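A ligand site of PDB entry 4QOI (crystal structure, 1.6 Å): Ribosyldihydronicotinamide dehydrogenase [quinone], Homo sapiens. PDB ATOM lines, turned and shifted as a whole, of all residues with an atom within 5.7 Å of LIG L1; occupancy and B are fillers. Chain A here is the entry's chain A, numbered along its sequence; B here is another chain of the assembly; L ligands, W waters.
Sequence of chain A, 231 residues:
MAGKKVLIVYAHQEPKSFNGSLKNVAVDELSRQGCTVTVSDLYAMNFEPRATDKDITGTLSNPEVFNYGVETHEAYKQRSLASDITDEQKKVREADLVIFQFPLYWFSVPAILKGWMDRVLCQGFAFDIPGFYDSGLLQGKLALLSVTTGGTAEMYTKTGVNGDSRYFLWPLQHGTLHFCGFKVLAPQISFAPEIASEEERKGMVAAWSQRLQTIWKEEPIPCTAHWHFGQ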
ATOM      1  N   HIS A  12      34.235  -4.616   9.793  1.00  0.00           N
ATOM      2  CA  HIS A  12      34.258  -4.778  11.248  1.00  0.00           C
ATOM      3  C   HIS A  12      35.293  -3.819  11.831  1.00  0.00           C
ATOM      4  O   HIS A  12      36.345  -3.594  11.222  1.00  0.00           O
ATOM      5  CB  HIS A  12      34.524  -6.219  11.702  1.00  0.00           C
ATOM      6  CG  HIS A  12      34.032  -6.470  13.096  1.00  0.00           C
ATOM      7  ND1 HIS A  12      34.673  -5.934  14.198  1.00  0.00           N
ATOM      8  CD2 HIS A  12      32.964  -7.202  13.517  1.00  0.00           C
ATOM      9  CE1 HIS A  12      33.964  -6.326  15.259  1.00  0.00           C
ATOM     10  NE2 HIS A  12      32.931  -7.106  14.898  1.00  0.00           N
ATOM     11  N   SER A  17      38.294  -9.297  16.502  1.00  0.00           N
ATOM     12  CA  SER A  17      36.958  -9.891  16.515  1.00  0.00           C
ATOM     13  C   SER A  17      36.892 -11.222  15.795  1.00  0.00           C
ATOM     14  O   SER A  17      37.782 -11.585  15.016  1.00  0.00           O
ATOM     15  CB  SER A  17      35.957  -8.944  15.869  1.00  0.00           C
ATOM     16  OG  SER A  17      36.230  -8.825  14.475  1.00  0.00           O
ATOM     17  N   PHE A  18      35.762 -11.919  15.995  1.00  0.00           N
ATOM     18  CA  PHE A  18      35.455 -13.143  15.294  1.00  0.00           C
ATOM     19  C   PHE A  18      35.383 -12.852  13.767  1.00  0.00           C
ATOM     20  O   PHE A  18      35.922 -13.630  12.969  1.00  0.00           O
ATOM     21  CB  PHE A  18      34.143 -13.711  15.811  1.00  0.00           C
ATOM     22  CG  PHE A  18      33.716 -14.992  15.152  1.00  0.00           C
ATOM     23  CD1 PHE A  18      34.333 -16.203  15.445  1.00  0.00           C
ATOM     24  CD2 PHE A  18      32.682 -14.990  14.219  1.00  0.00           C
ATOM     25  CE1 PHE A  18      33.934 -17.374  14.812  1.00  0.00           C
ATOM     26  CE2 PHE A  18      32.271 -16.173  13.611  1.00  0.00           C
ATOM     27  CZ  PHE A  18      32.901 -17.354  13.912  1.00  0.00           C
ATOM     28  N   ASN A  19      34.794 -11.692  13.376  1.00  0.00           N
ATOM     29  CA  ASN A  19      34.787 -11.316  11.946  1.00  0.00           C
ATOM     30  C   ASN A  19      36.223 -11.161  11.439  1.00  0.00           C
ATOM     31  O   ASN A  19      36.536 -11.589  10.335  1.00  0.00           O
ATOM     32  CB  ASN A  19      34.024 -10.003  11.721  1.00  0.00           C
ATOM     33  CG  ASN A  19      32.583 -10.267  11.436  1.00  0.00           C
ATOM     34  OD1 ASN A  19      32.171 -10.355  10.282  1.00  0.00           O
ATOM     35  ND2 ASN A  19      31.769 -10.415  12.494  1.00  0.00           N
ATOM     36  N   GLY A  20      37.076 -10.555  12.274  1.00  0.00           N
ATOM     37  CA  GLY A  20      38.489 -10.386  11.946  1.00  0.00           C
ATOM     38  C   GLY A  20      39.145 -11.746  11.697  1.00  0.00           C
ATOM     39  O   GLY A  20      39.886 -11.938  10.714  1.00  0.00           O
ATOM     40  N   PHE A 102      30.954  -9.659   7.200  1.00  0.00           N
ATOM     41  CA  PHE A 102      30.370  -8.660   8.088  1.00  0.00           C
ATOM     42  C   PHE A 102      29.494  -9.269   9.148  1.00  0.00           C
ATOM     43  O   PHE A 102      28.902 -10.359   8.930  1.00  0.00           O
ATOM     44  CB  PHE A 102      29.476  -7.706   7.234  1.00  0.00           C
ATOM     45  CG  PHE A 102      28.348  -8.388   6.485  1.00  0.00           C
ATOM     46  CD1 PHE A 102      28.566  -8.975   5.248  1.00  0.00           C
ATOM     47  CD2 PHE A 102      27.047  -8.379   6.982  1.00  0.00           C
ATOM     48  CE1 PHE A 102      27.520  -9.593   4.547  1.00  0.00           C
ATOM     49  CE2 PHE A 102      26.015  -9.027   6.307  1.00  0.00           C
ATOM     50  CZ  PHE A 102      26.257  -9.594   5.062  1.00  0.00           C
ATOM     51  N   PRO A 103      29.326  -8.511  10.246  1.00  0.00           N
ATOM     52  CA  PRO A 103      28.304  -8.899  11.241  1.00  0.00           C
ATOM     53  C   PRO A 103      26.921  -8.409  10.747  1.00  0.00           C
ATOM     54  O   PRO A 103      26.799  -7.323  10.180  1.00  0.00           O
ATOM     55  CB  PRO A 103      28.704  -8.096  12.485  1.00  0.00           C
ATOM     56  CG  PRO A 103      29.421  -6.842  11.940  1.00  0.00           C
ATOM     57  CD  PRO A 103      30.033  -7.262  10.610  1.00  0.00           C
ATOM     58  N   LEU A 104      25.870  -9.209  11.008  1.00  0.00           N
ATOM     59  CA  LEU A 104      24.517  -8.790  10.627  1.00  0.00           C
ATOM     60  C   LEU A 104      24.102  -7.623  11.515  1.00  0.00           C
ATOM     61  O   LEU A 104      24.211  -7.729  12.749  1.00  0.00           O
ATOM     62  CB  LEU A 104      23.553  -9.963  10.861  1.00  0.00           C
ATOM     63  CG  LEU A 104      22.166  -9.868  10.222  1.00  0.00           C
ATOM     64  CD1 LEU A 104      22.265  -9.954   8.690  1.00  0.00           C
ATOM     65  CD2 LEU A 104      21.287 -11.051  10.691  1.00  0.00           C
ATOM     66  N   TYR A 105      23.646  -6.529  10.890  1.00  0.00           N
ATOM     67  CA  TYR A 105      23.133  -5.344  11.601  1.00  0.00           C
ATOM     68  C   TYR A 105      21.717  -5.139  11.106  1.00  0.00           C
ATOM     69  O   TYR A 105      21.498  -4.838   9.920  1.00  0.00           O
ATOM     70  CB  TYR A 105      23.949  -4.077  11.277  1.00  0.00           C
ATOM     71  CG  TYR A 105      25.173  -3.784  12.121  1.00  0.00           C
ATOM     72  CD1 TYR A 105      25.858  -4.806  12.783  1.00  0.00           C
ATOM     73  CD2 TYR A 105      25.739  -2.512  12.123  1.00  0.00           C
ATOM     74  CE1 TYR A 105      27.020  -4.546  13.500  1.00  0.00           C
ATOM     75  CE2 TYR A 105      26.909  -2.235  12.827  1.00  0.00           C
ATOM     76  CZ  TYR A 105      27.560  -3.256  13.501  1.00  0.00           C
ATOM     77  OH  TYR A 105      28.665  -2.910  14.210  1.00  0.00           O
ATOM     78  N   TRP A 106      20.745  -5.286  11.998  1.00  0.00           N
ATOM     79  CA  TRP A 106      19.360  -5.094  11.607  1.00  0.00           C
ATOM     80  C   TRP A 106      18.963  -5.897  10.372  1.00  0.00           C
ATOM     81  O   TRP A 106      18.407  -5.330   9.419  1.00  0.00           O
ATOM     82  CB  TRP A 106      19.022  -3.600  11.469  1.00  0.00           C
ATOM     83  CG  TRP A 106      19.113  -2.891  12.780  1.00  0.00           C
ATOM     84  CD1 TRP A 106      19.932  -1.859  13.114  1.00  0.00           C
ATOM     85  CD2 TRP A 106      18.325  -3.168  13.950  1.00  0.00           C
ATOM     86  NE1 TRP A 106      19.709  -1.475  14.428  1.00  0.00           N
ATOM     87  CE2 TRP A 106      18.745  -2.290  14.967  1.00  0.00           C
ATOM     88  CE3 TRP A 106      17.345  -4.134  14.243  1.00  0.00           C
ATOM     89  CZ2 TRP A 106      18.175  -2.303  16.240  1.00  0.00           C
ATOM     90  CZ3 TRP A 106      16.758  -4.126  15.502  1.00  0.00           C
ATOM     91  CH2 TRP A 106      17.205  -3.248  16.487  1.00  0.00           C
ATOM     92  N   PHE A 107      19.258  -7.214  10.395  1.00  0.00           N
ATOM     93  CA  PHE A 107      18.924  -8.175   9.322  1.00  0.00           C
ATOM     94  C   PHE A 107      19.546  -7.768   7.984  1.00  0.00           C
ATOM     95  O   PHE A 107      19.079  -8.204   6.930  1.00  0.00           O
ATOM     96  CB  PHE A 107      17.394  -8.305   9.151  1.00  0.00           C
ATOM     97  CG  PHE A 107      16.661  -9.279  10.045  1.00  0.00           C
ATOM     98  CD1 PHE A 107      17.196  -9.681  11.259  1.00  0.00           C
ATOM     99  CD2 PHE A 107      15.414  -9.793   9.667  1.00  0.00           C
ATOM    100  CE1 PHE A 107      16.508 -10.592  12.076  1.00  0.00           C
ATOM    101  CE2 PHE A 107      14.725 -10.676  10.496  1.00  0.00           C
ATOM    102  CZ  PHE A 107      15.276 -11.067  11.694  1.00  0.00           C
ATOM    103  N   SER A 108      20.596  -6.941   8.032  1.00  0.00           N
ATOM    104  CA  SER A 108      21.232  -6.422   6.811  1.00  0.00           C
ATOM    105  C   SER A 108      22.704  -6.164   7.053  1.00  0.00           C
ATOM    106  O   SER A 108      23.285  -6.671   8.021  1.00  0.00           O
ATOM    107  CB  SER A 108      20.504  -5.140   6.369  1.00  0.00           C
ATOM    108  OG  SER A 108      20.985  -4.550   5.155  1.00  0.00           O
ATOM    109  N   THR A 148      27.957 -13.029  10.197  1.00  0.00           N
ATOM    110  CA  THR A 148      27.974 -13.480  11.597  1.00  0.00           C
ATOM    111  C   THR A 148      26.721 -12.906  12.253  1.00  0.00           C
ATOM    112  O   THR A 148      26.294 -11.804  11.884  1.00  0.00           O
ATOM    113  CB  THR A 148      29.251 -13.085  12.343  1.00  0.00           C
ATOM    114  OG1 THR A 148      29.289 -11.670  12.533  1.00  0.00           O
ATOM    115  CG2 THR A 148      30.510 -13.507  11.607  1.00  0.00           C
ATOM    116  N   THR A 149      26.117 -13.633  13.228  1.00  0.00           N
ATOM    117  CA  THR A 149      24.891 -13.131  13.860  1.00  0.00           C
ATOM    118  C   THR A 149      24.961 -13.105  15.370  1.00  0.00           C
ATOM    119  O   THR A 149      25.795 -13.803  15.949  1.00  0.00           O
ATOM    120  CB  THR A 149      23.695 -14.025  13.478  1.00  0.00           C
ATOM    121  OG1 THR A 149      23.876 -15.315  14.087  1.00  0.00           O
ATOM    122  CG2 THR A 149      23.524 -14.194  11.955  1.00  0.00           C
ATOM    123  N   GLY A 150      24.048 -12.363  15.994  1.00  0.00           N
ATOM    124  CA  GLY A 150      23.865 -12.423  17.433  1.00  0.00           C
ATOM    125  C   GLY A 150      22.948 -13.598  17.756  1.00  0.00           C
ATOM    126  O   GLY A 150      23.206 -14.343  18.704  1.00  0.00           O
ATOM    127  N   GLY A 151      21.869 -13.755  16.982  1.00  0.00           N
ATOM    128  CA  GLY A 151      20.884 -14.829  17.143  1.00  0.00           C
ATOM    129  C   GLY A 151      21.385 -16.216  16.789  1.00  0.00           C
ATOM    130  O   GLY A 151      22.258 -16.387  15.929  1.00  0.00           O
ATOM    131  N   TYR A 156      16.798 -18.378  13.805  1.00  0.00           N
ATOM    132  CA  TYR A 156      16.686 -18.161  12.385  1.00  0.00           C
ATOM    133  C   TYR A 156      16.128 -19.354  11.596  1.00  0.00           C
ATOM    134  O   TYR A 156      16.685 -19.716  10.608  1.00  0.00           O
ATOM    135  CB  TYR A 156      18.042 -17.709  11.804  1.00  0.00           C
ATOM    136  CG  TYR A 156      18.394 -16.280  12.157  1.00  0.00           C
ATOM    137  CD1 TYR A 156      17.797 -15.235  11.539  1.00  0.00           C
ATOM    138  CD2 TYR A 156      19.312 -16.013  13.112  1.00  0.00           C
ATOM    139  CE1 TYR A 156      18.120 -13.938  11.875  1.00  0.00           C
ATOM    140  CE2 TYR A 156      19.631 -14.733  13.471  1.00  0.00           C
ATOM    141  CZ  TYR A 156      19.035 -13.693  12.831  1.00  0.00           C
ATOM    142  OH  TYR A 156      19.357 -12.413  13.198  1.00  0.00           O
ATOM    143  N   ASN A 162      12.943 -15.033  14.484  1.00  0.00           N
ATOM    144  CA  ASN A 162      13.511 -14.202  13.420  1.00  0.00           C
ATOM    145  C   ASN A 162      13.098 -14.656  12.037  1.00  0.00           C
ATOM    146  O   ASN A 162      13.381 -13.953  11.070  1.00  0.00           O
ATOM    147  CB  ASN A 162      15.033 -14.175  13.536  1.00  0.00           C
ATOM    148  CG  ASN A 162      15.578 -13.487  14.765  1.00  0.00           C
ATOM    149  OD1 ASN A 162      14.940 -12.650  15.399  1.00  0.00           O
ATOM    150  ND2 ASN A 162      16.793 -13.838  15.136  1.00  0.00           N
ATOM    151  N   PRO A 193      28.522 -16.320  17.469  1.00  0.00           N
ATOM    152  CA  PRO A 193      29.865 -16.576  18.010  1.00  0.00           C
ATOM    153  C   PRO A 193      30.123 -16.047  19.422  1.00  0.00           C
ATOM    154  O   PRO A 193      30.867 -16.688  20.164  1.00  0.00           O
ATOM    155  CB  PRO A 193      30.778 -15.900  16.983  1.00  0.00           C
ATOM    156  CG  PRO A 193      29.928 -14.827  16.373  1.00  0.00           C
ATOM    157  CD  PRO A 193      28.606 -15.498  16.239  1.00  0.00           C
ATOM    158  N   GLU A 194      29.550 -14.888  19.802  1.00  0.00           N
ATOM    159  CA  GLU A 194      29.809 -14.292  21.120  1.00  0.00           C
ATOM    160  C   GLU A 194      29.262 -15.131  22.283  1.00  0.00           C
ATOM    161  O   GLU A 194      29.798 -15.040  23.381  1.00  0.00           O
ATOM    162  CB  GLU A 194      29.316 -12.848  21.186  1.00  0.00           C
ATOM    163  CG  GLU A 194      29.949 -11.977  20.110  1.00  0.00           C
ATOM    164  CD  GLU A 194      29.849 -10.472  20.280  1.00  0.00           C
ATOM    165  OE1 GLU A 194      29.064  -9.993  21.133  1.00  0.00           O
ATOM    166  OE2 GLU A 194      30.600  -9.765  19.580  1.00  0.00           O
ATOM    167  N   ASN B  67      33.833  -3.796  21.073  1.00  0.00           N
ATOM    168  CA  ASN B  67      32.583  -4.471  20.731  1.00  0.00           C
ATOM    169  C   ASN B  67      31.522  -3.384  20.690  1.00  0.00           C
ATOM    170  O   ASN B  67      31.111  -2.864  21.738  1.00  0.00           O
ATOM    171  CB  ASN B  67      32.251  -5.568  21.771  1.00  0.00           C
ATOM    172  CG  ASN B  67      31.029  -6.393  21.455  1.00  0.00           C
ATOM    173  OD1 ASN B  67      29.928  -5.878  21.189  1.00  0.00           O
ATOM    174  ND2 ASN B  67      31.165  -7.705  21.569  1.00  0.00           N
ATOM    175  N   TYR B  68      31.137  -2.975  19.475  1.00  0.00           N
ATOM    176  CA  TYR B  68      30.182  -1.875  19.310  1.00  0.00           C
ATOM    177  C   TYR B  68      28.880  -2.052  20.097  1.00  0.00           C
ATOM    178  O   TYR B  68      28.450  -1.112  20.788  1.00  0.00           O
ATOM    179  CB  TYR B  68      29.895  -1.617  17.806  1.00  0.00           C
ATOM    180  CG  TYR B  68      29.091  -0.348  17.594  1.00  0.00           C
ATOM    181  CD1 TYR B  68      29.703   0.908  17.610  1.00  0.00           C
ATOM    182  CD2 TYR B  68      27.708  -0.401  17.447  1.00  0.00           C
ATOM    183  CE1 TYR B  68      28.968   2.076  17.432  1.00  0.00           C
ATOM    184  CE2 TYR B  68      26.959   0.765  17.274  1.00  0.00           C
ATOM    185  CZ  TYR B  68      27.594   2.003  17.280  1.00  0.00           C
ATOM    186  OH  TYR B  68      26.853   3.142  17.178  1.00  0.00           O
ATOM    187  N   GLY B  69      28.271  -3.237  20.020  1.00  0.00           N
ATOM    188  CA  GLY B  69      27.030  -3.506  20.738  1.00  0.00           C
ATOM    189  C   GLY B  69      27.171  -3.382  22.237  1.00  0.00           C
ATOM    190  O   GLY B  69      26.342  -2.740  22.901  1.00  0.00           O
ATOM    191  N   MET B 117      19.535   3.830  11.828  1.00  0.00           N
ATOM    192  CA  MET B 117      19.009   2.633  12.508  1.00  0.00           C
ATOM    193  C   MET B 117      20.090   1.947  13.318  1.00  0.00           C
ATOM    194  O   MET B 117      19.843   1.576  14.467  1.00  0.00           O
ATOM    195  CB  MET B 117      18.404   1.680  11.471  1.00  0.00           C
ATOM    196  CG  MET B 117      17.319   2.367  10.716  1.00  0.00           C
ATOM    197  SD  MET B 117      16.739   1.406   9.360  1.00  0.00           S
ATOM    198  CE  MET B 117      15.010   2.080   9.266  1.00  0.00           C
ATOM    199  N   ASP B 118      21.284   1.786  12.746  1.00  0.00           N
ATOM    200  CA  ASP B 118      22.357   1.114  13.473  1.00  0.00           C
ATOM    201  C   ASP B 118      22.780   1.809  14.747  1.00  0.00           C
ATOM    202  O   ASP B 118      23.101   1.140  15.739  1.00  0.00           O
ATOM    203  CB  ASP B 118      23.611   0.984  12.593  1.00  0.00           C
ATOM    204  CG  ASP B 118      23.445   0.166  11.337  1.00  0.00           C
ATOM    205  OD1 ASP B 118      22.438  -0.592  11.233  1.00  0.00           O
ATOM    206  OD2 ASP B 118      24.333   0.241  10.473  1.00  0.00           O
ATOM    207  N   ARG B 119      22.854   3.174  14.698  1.00  0.00           N
ATOM    208  CA  ARG B 119      23.408   3.941  15.799  1.00  0.00           C
ATOM    209  C   ARG B 119      22.358   4.411  16.801  1.00  0.00           C
ATOM    210  O   ARG B 119      22.659   4.545  17.987  1.00  0.00           O
ATOM    211  CB  ARG B 119      24.176   5.169  15.234  1.00  0.00           C
ATOM    212  CG  ARG B 119      25.385   4.743  14.378  1.00  0.00           C
ATOM    213  CD  ARG B 119      26.033   5.934  13.653  1.00  0.00           C
ATOM    214  NE  ARG B 119      26.725   6.799  14.612  1.00  0.00           N
ATOM    215  CZ  ARG B 119      26.422   8.071  14.888  1.00  0.00           C
ATOM    216  NH1 ARG B 119      25.473   8.700  14.188  1.00  0.00           N
ATOM    217  NH2 ARG B 119      27.095   8.735  15.824  1.00  0.00           N
ATOM    218  N   GLY B 175      12.584  -7.207  11.152  1.00  0.00           N
ATOM    219  CA  GLY B 175      13.892  -7.289  11.767  1.00  0.00           C
ATOM    220  C   GLY B 175      14.284  -6.047  12.545  1.00  0.00           C
ATOM    221  O   GLY B 175      15.098  -6.135  13.458  1.00  0.00           O
HETATM  222  N1  LIG L   1      22.447  -9.950  15.401  1.00  0.00           N
HETATM  223  C1  LIG L   1      21.408 -10.618  14.780  1.00  0.00           C
HETATM  224  O1  LIG L   1      21.267 -11.849  14.903  1.00  0.00           O
HETATM  225  N2  LIG L   1      20.506  -9.888  14.004  1.00  0.00           N
HETATM  226  C2  LIG L   1      20.514  -8.506  13.820  1.00  0.00           C
HETATM  227  O2  LIG L   1      19.712  -7.964  13.061  1.00  0.00           O
HETATM  228  C3  LIG L   1      21.566  -7.806  14.512  1.00  0.00           C
HETATM  229  N3  LIG L   1      21.593  -6.489  14.435  1.00  0.00           N
HETATM  230  C4  LIG L   1      22.644  -5.827  15.062  1.00  0.00           C
HETATM  231  C5  LIG L   1      22.701  -4.432  14.978  1.00  0.00           C
HETATM  232  C6  LIG L   1      23.739  -3.710  15.559  1.00  0.00           C
HETATM  233  C7  LIG L   1      23.781  -2.210  15.400  1.00  0.00           C
HETATM  234  C8  LIG L   1      24.733  -4.401  16.293  1.00  0.00           C
HETATM  235  C9  LIG L   1      25.889  -3.674  16.927  1.00  0.00           C
HETATM  236  C10 LIG L   1      24.665  -5.784  16.393  1.00  0.00           C
HETATM  237  C11 LIG L   1      23.644  -6.514  15.773  1.00  0.00           C
HETATM  238  N4  LIG L   1      23.544  -7.938  15.871  1.00  0.00           N
HETATM  239  C12 LIG L   1      22.519  -8.613  15.266  1.00  0.00           C
HETATM  240  C13 LIG L   1      24.561  -8.691  16.616  1.00  0.00           C
HETATM  241  C14 LIG L   1      25.786  -8.902  15.721  1.00  0.00           C
HETATM  242  O3  LIG L   1      25.418  -9.462  14.455  1.00  0.00           O
HETATM  243  C15 LIG L   1      26.783  -9.820  16.433  1.00  0.00           C
HETATM  244  O4  LIG L   1      27.195  -9.147  17.625  1.00  0.00           O
HETATM  245  C16 LIG L   1      28.011 -10.122  15.587  1.00  0.00           C
HETATM  246  O5  LIG L   1      27.638 -10.811  14.391  1.00  0.00           O
HETATM  247  C17 LIG L   1      29.039 -10.931  16.335  1.00  0.00           C
HETATM  248  O6  LIG L   1      30.247 -10.997  15.549  1.00  0.00           O
HETATM  249  P1  LIG L   1      31.573 -10.214  16.071  1.00  0.00           P
HETATM  250  O7  LIG L   1      31.845 -10.824  17.488  1.00  0.00           O
HETATM  251  O8  LIG L   1      31.210  -8.753  16.229  1.00  0.00           O
HETATM  252  O9  LIG L   1      32.740 -10.510  15.162  1.00  0.00           O
HETATM  253  C1  LG2 L   2      20.542 -10.679  19.762  1.00  0.00           C
HETATM  254  C2  LG2 L   2      19.016  -9.051  16.900  1.00  0.00           C
HETATM  255  C3  LG2 L   2      23.663  -4.730  19.760  1.00  0.00           C
HETATM  256  C4  LG2 L   2      20.184 -12.581  21.286  1.00  0.00           C
HETATM  257  C5  LG2 L   2      20.364 -14.058  21.461  1.00  0.00           C
HETATM  258  C6  LG2 L   2      20.615 -10.557  18.260  1.00  0.00           C
HETATM  259  C7  LG2 L   2      20.626  -7.970  18.023  1.00  0.00           C
HETATM  260  C8  LG2 L   2      21.721  -7.549  18.762  1.00  0.00           C
HETATM  261  C9  LG2 L   2      20.226  -5.686  17.274  1.00  0.00           C
HETATM  262  C10 LG2 L   2      19.879  -7.029  17.296  1.00  0.00           C
HETATM  263  C11 LG2 L   2      20.056  -9.259  17.746  1.00  0.00           C
HETATM  264  C12 LG2 L   2      22.072  -6.206  18.749  1.00  0.00           C
HETATM  265  C13 LG2 L   2      21.341  -5.282  17.993  1.00  0.00           C
HETATM  266  N1  LG2 L   2      20.787 -12.046  20.217  1.00  0.00           N
HETATM  267  N2  LG2 L   2      18.907  -7.718  16.618  1.00  0.00           N
HETATM  268  O1  LG2 L   2      23.153  -6.040  19.576  1.00  0.00           O
HETATM  269  O2  LG2 L   2      19.506 -11.913  22.045  1.00  0.00           O
HETATM  270  O   HOH W   1      27.054 -10.775  19.594  1.00  0.00           O
HETATM  271  O   HOH W   2      29.369  -6.661  15.719  1.00  0.00           O
HETATM  272  O   HOH W   3      34.286 -11.317  18.385  1.00  0.00           O
HETATM  273  O   HOH W   4      31.668  -7.222  18.402  1.00  0.00           O
HETATM  274  O   HOH W   5      26.528  -6.873  18.933  1.00  0.00           O
HETATM  275  O   HOH W   6      21.725  -1.037  17.133  1.00  0.00           O
HETATM  276  O   HOH W   7      23.285  -1.917  18.781  1.00  0.00           O
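The side-chain hydroxyl (OH) of Tyr 156 is in hydrogen-bond range of an oxygen (O1) of LIG L1, at 2.6 Å. O of Thr 148 lies within hydrogen-bond range of O5 of LIG L1 (3.0 Å). The side-chain hydroxyl (OG1) of Thr 148 sits at hydrogen-bond distance from an oxygen (O5) of LIG L1, 2.6 Å away. OE2 of Glu 194 sits close to O7 of LIG L1. N of Leu 104 is in hydrogen-bond range of O3 of LIG L1 (3.5 Å). The backbone carbonyl oxygen (O) of Leu 104 is in hydrogen-bond range of an oxygen (O3) of LIG L1. NE2 of His 12 sits at hydrogen-bond distance from O8 of LIG L1 (2.7 Å). N of Phe 107 is in hydrogen-bond range of O2 of LIG L1 (2.8 Å). The backbone NH (N) of Asn 19 lies within hydrogen-bond range of an oxygen (O9) of LIG L1, 3.0 Å away. O9 of LIG L1 is in hydrogen-bond range of ND2 of Asn 19 (2.8 Å). The backbone NH of Trp 106 lies within hydrogen-bond range of a nitrogen (N3) of LIG L1, at 2.8 Å. An oxygen (O1) of LIG L1 is in hydrogen-bond range of the backbone NH (N) of Gly 151 (2.9 Å). The backbone NH of Gly 150 sits at hydrogen-bond distance from a nitrogen (N1) of LIG L1, 3.0 Å away. N of Thr 149 lies within hydrogen-bond range of O5 of LIG L1 (3.4 Å). N of Phe 18 lies within hydrogen-bond range of O9 of LIG L1, at 3.4 Å.
The side-chain hydroxyl (OG1) of Thr 148 is in hydrogen-bond range of the side-chain amide nitrogen (ND2) of Asn 19 (2.8 Å). The backbone NH of Thr 148 lies within hydrogen-bond range of the backbone carbonyl oxygen of Phe 102 (3.1 Å). A ring nitrogen (ND1) of His 12 is in hydrogen-bond range of the side-chain hydroxyl (OG) of Ser 17 (3.3 Å). The backbone NH of Phe 102 lies close to the side-chain amide oxygen of Asn 19. NE1 of Trp 106 is in hydrogen-bond range of O of Met 117 of chain B (3.1 Å). The side-chain hydroxyl (OG1) of Thr 149 is in hydrogen-bond range of the backbone carbonyl oxygen (O) of Gly 151, at 2.7 Å. The backbone NH of Gly 20 is in hydrogen-bond range of the side-chain hydroxyl of Ser 17. N of Gly 69 of chain B sits close to OD1 of Asn 67 of chain B (3.3 Å).
Residues that only touch LIG L1: Ser 17 (3.6 Å), Pro 103 (3.5 Å), Tyr 105 (3.4 Å), Pro 193 (3.9 Å), Tyr 68 of chain B (3.8 Å), Gly 69 of chain B (3.9 Å) and Asp 118 of chain B (3.4 Å). Hydrophobic or aromatic side chains that line LIG L1: His 12, Phe 18, Pro 103, Leu 104, Tyr 105, Phe 107, Tyr 156, Pro 193 and Tyr 68 of chain B. 19 residues have an atom within 4 Å of LIG L1: His 12, Ser 17, Phe 18, Asn 19, Pro 103, Leu 104, Tyr 105, Trp 106, Phe 107, Thr 148, Thr 149, Gly 150, Gly 151, Tyr 156, Pro 193, Glu 194, Tyr 68 of chain B, Gly 69 of chain B and Asp 118 of chain B. The nearest printed residue that does not touch LIG L1 is Asn 162 (4.9 Å).
Water W1 lies within hydrogen-bond range of an oxygen (O4) of LIG L1 (2.6 Å) and the side-chain carboxylate (OE1) of Glu 194 (2.6 Å). Water W3 bridges an oxygen (O7) of LIG L1 (2.6 Å) and the backbone NH of Phe 18 (2.9 Å). Water W4 lies within hydrogen-bond range of O8 of LIG L1, OE2 of Glu 194 and ND2 of Asn 67 of chain B. Water W6 lies within hydrogen-bond range of O of Asp 118 of chain B (2.9 Å) and NE1 of Trp 106 (3.4 Å).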
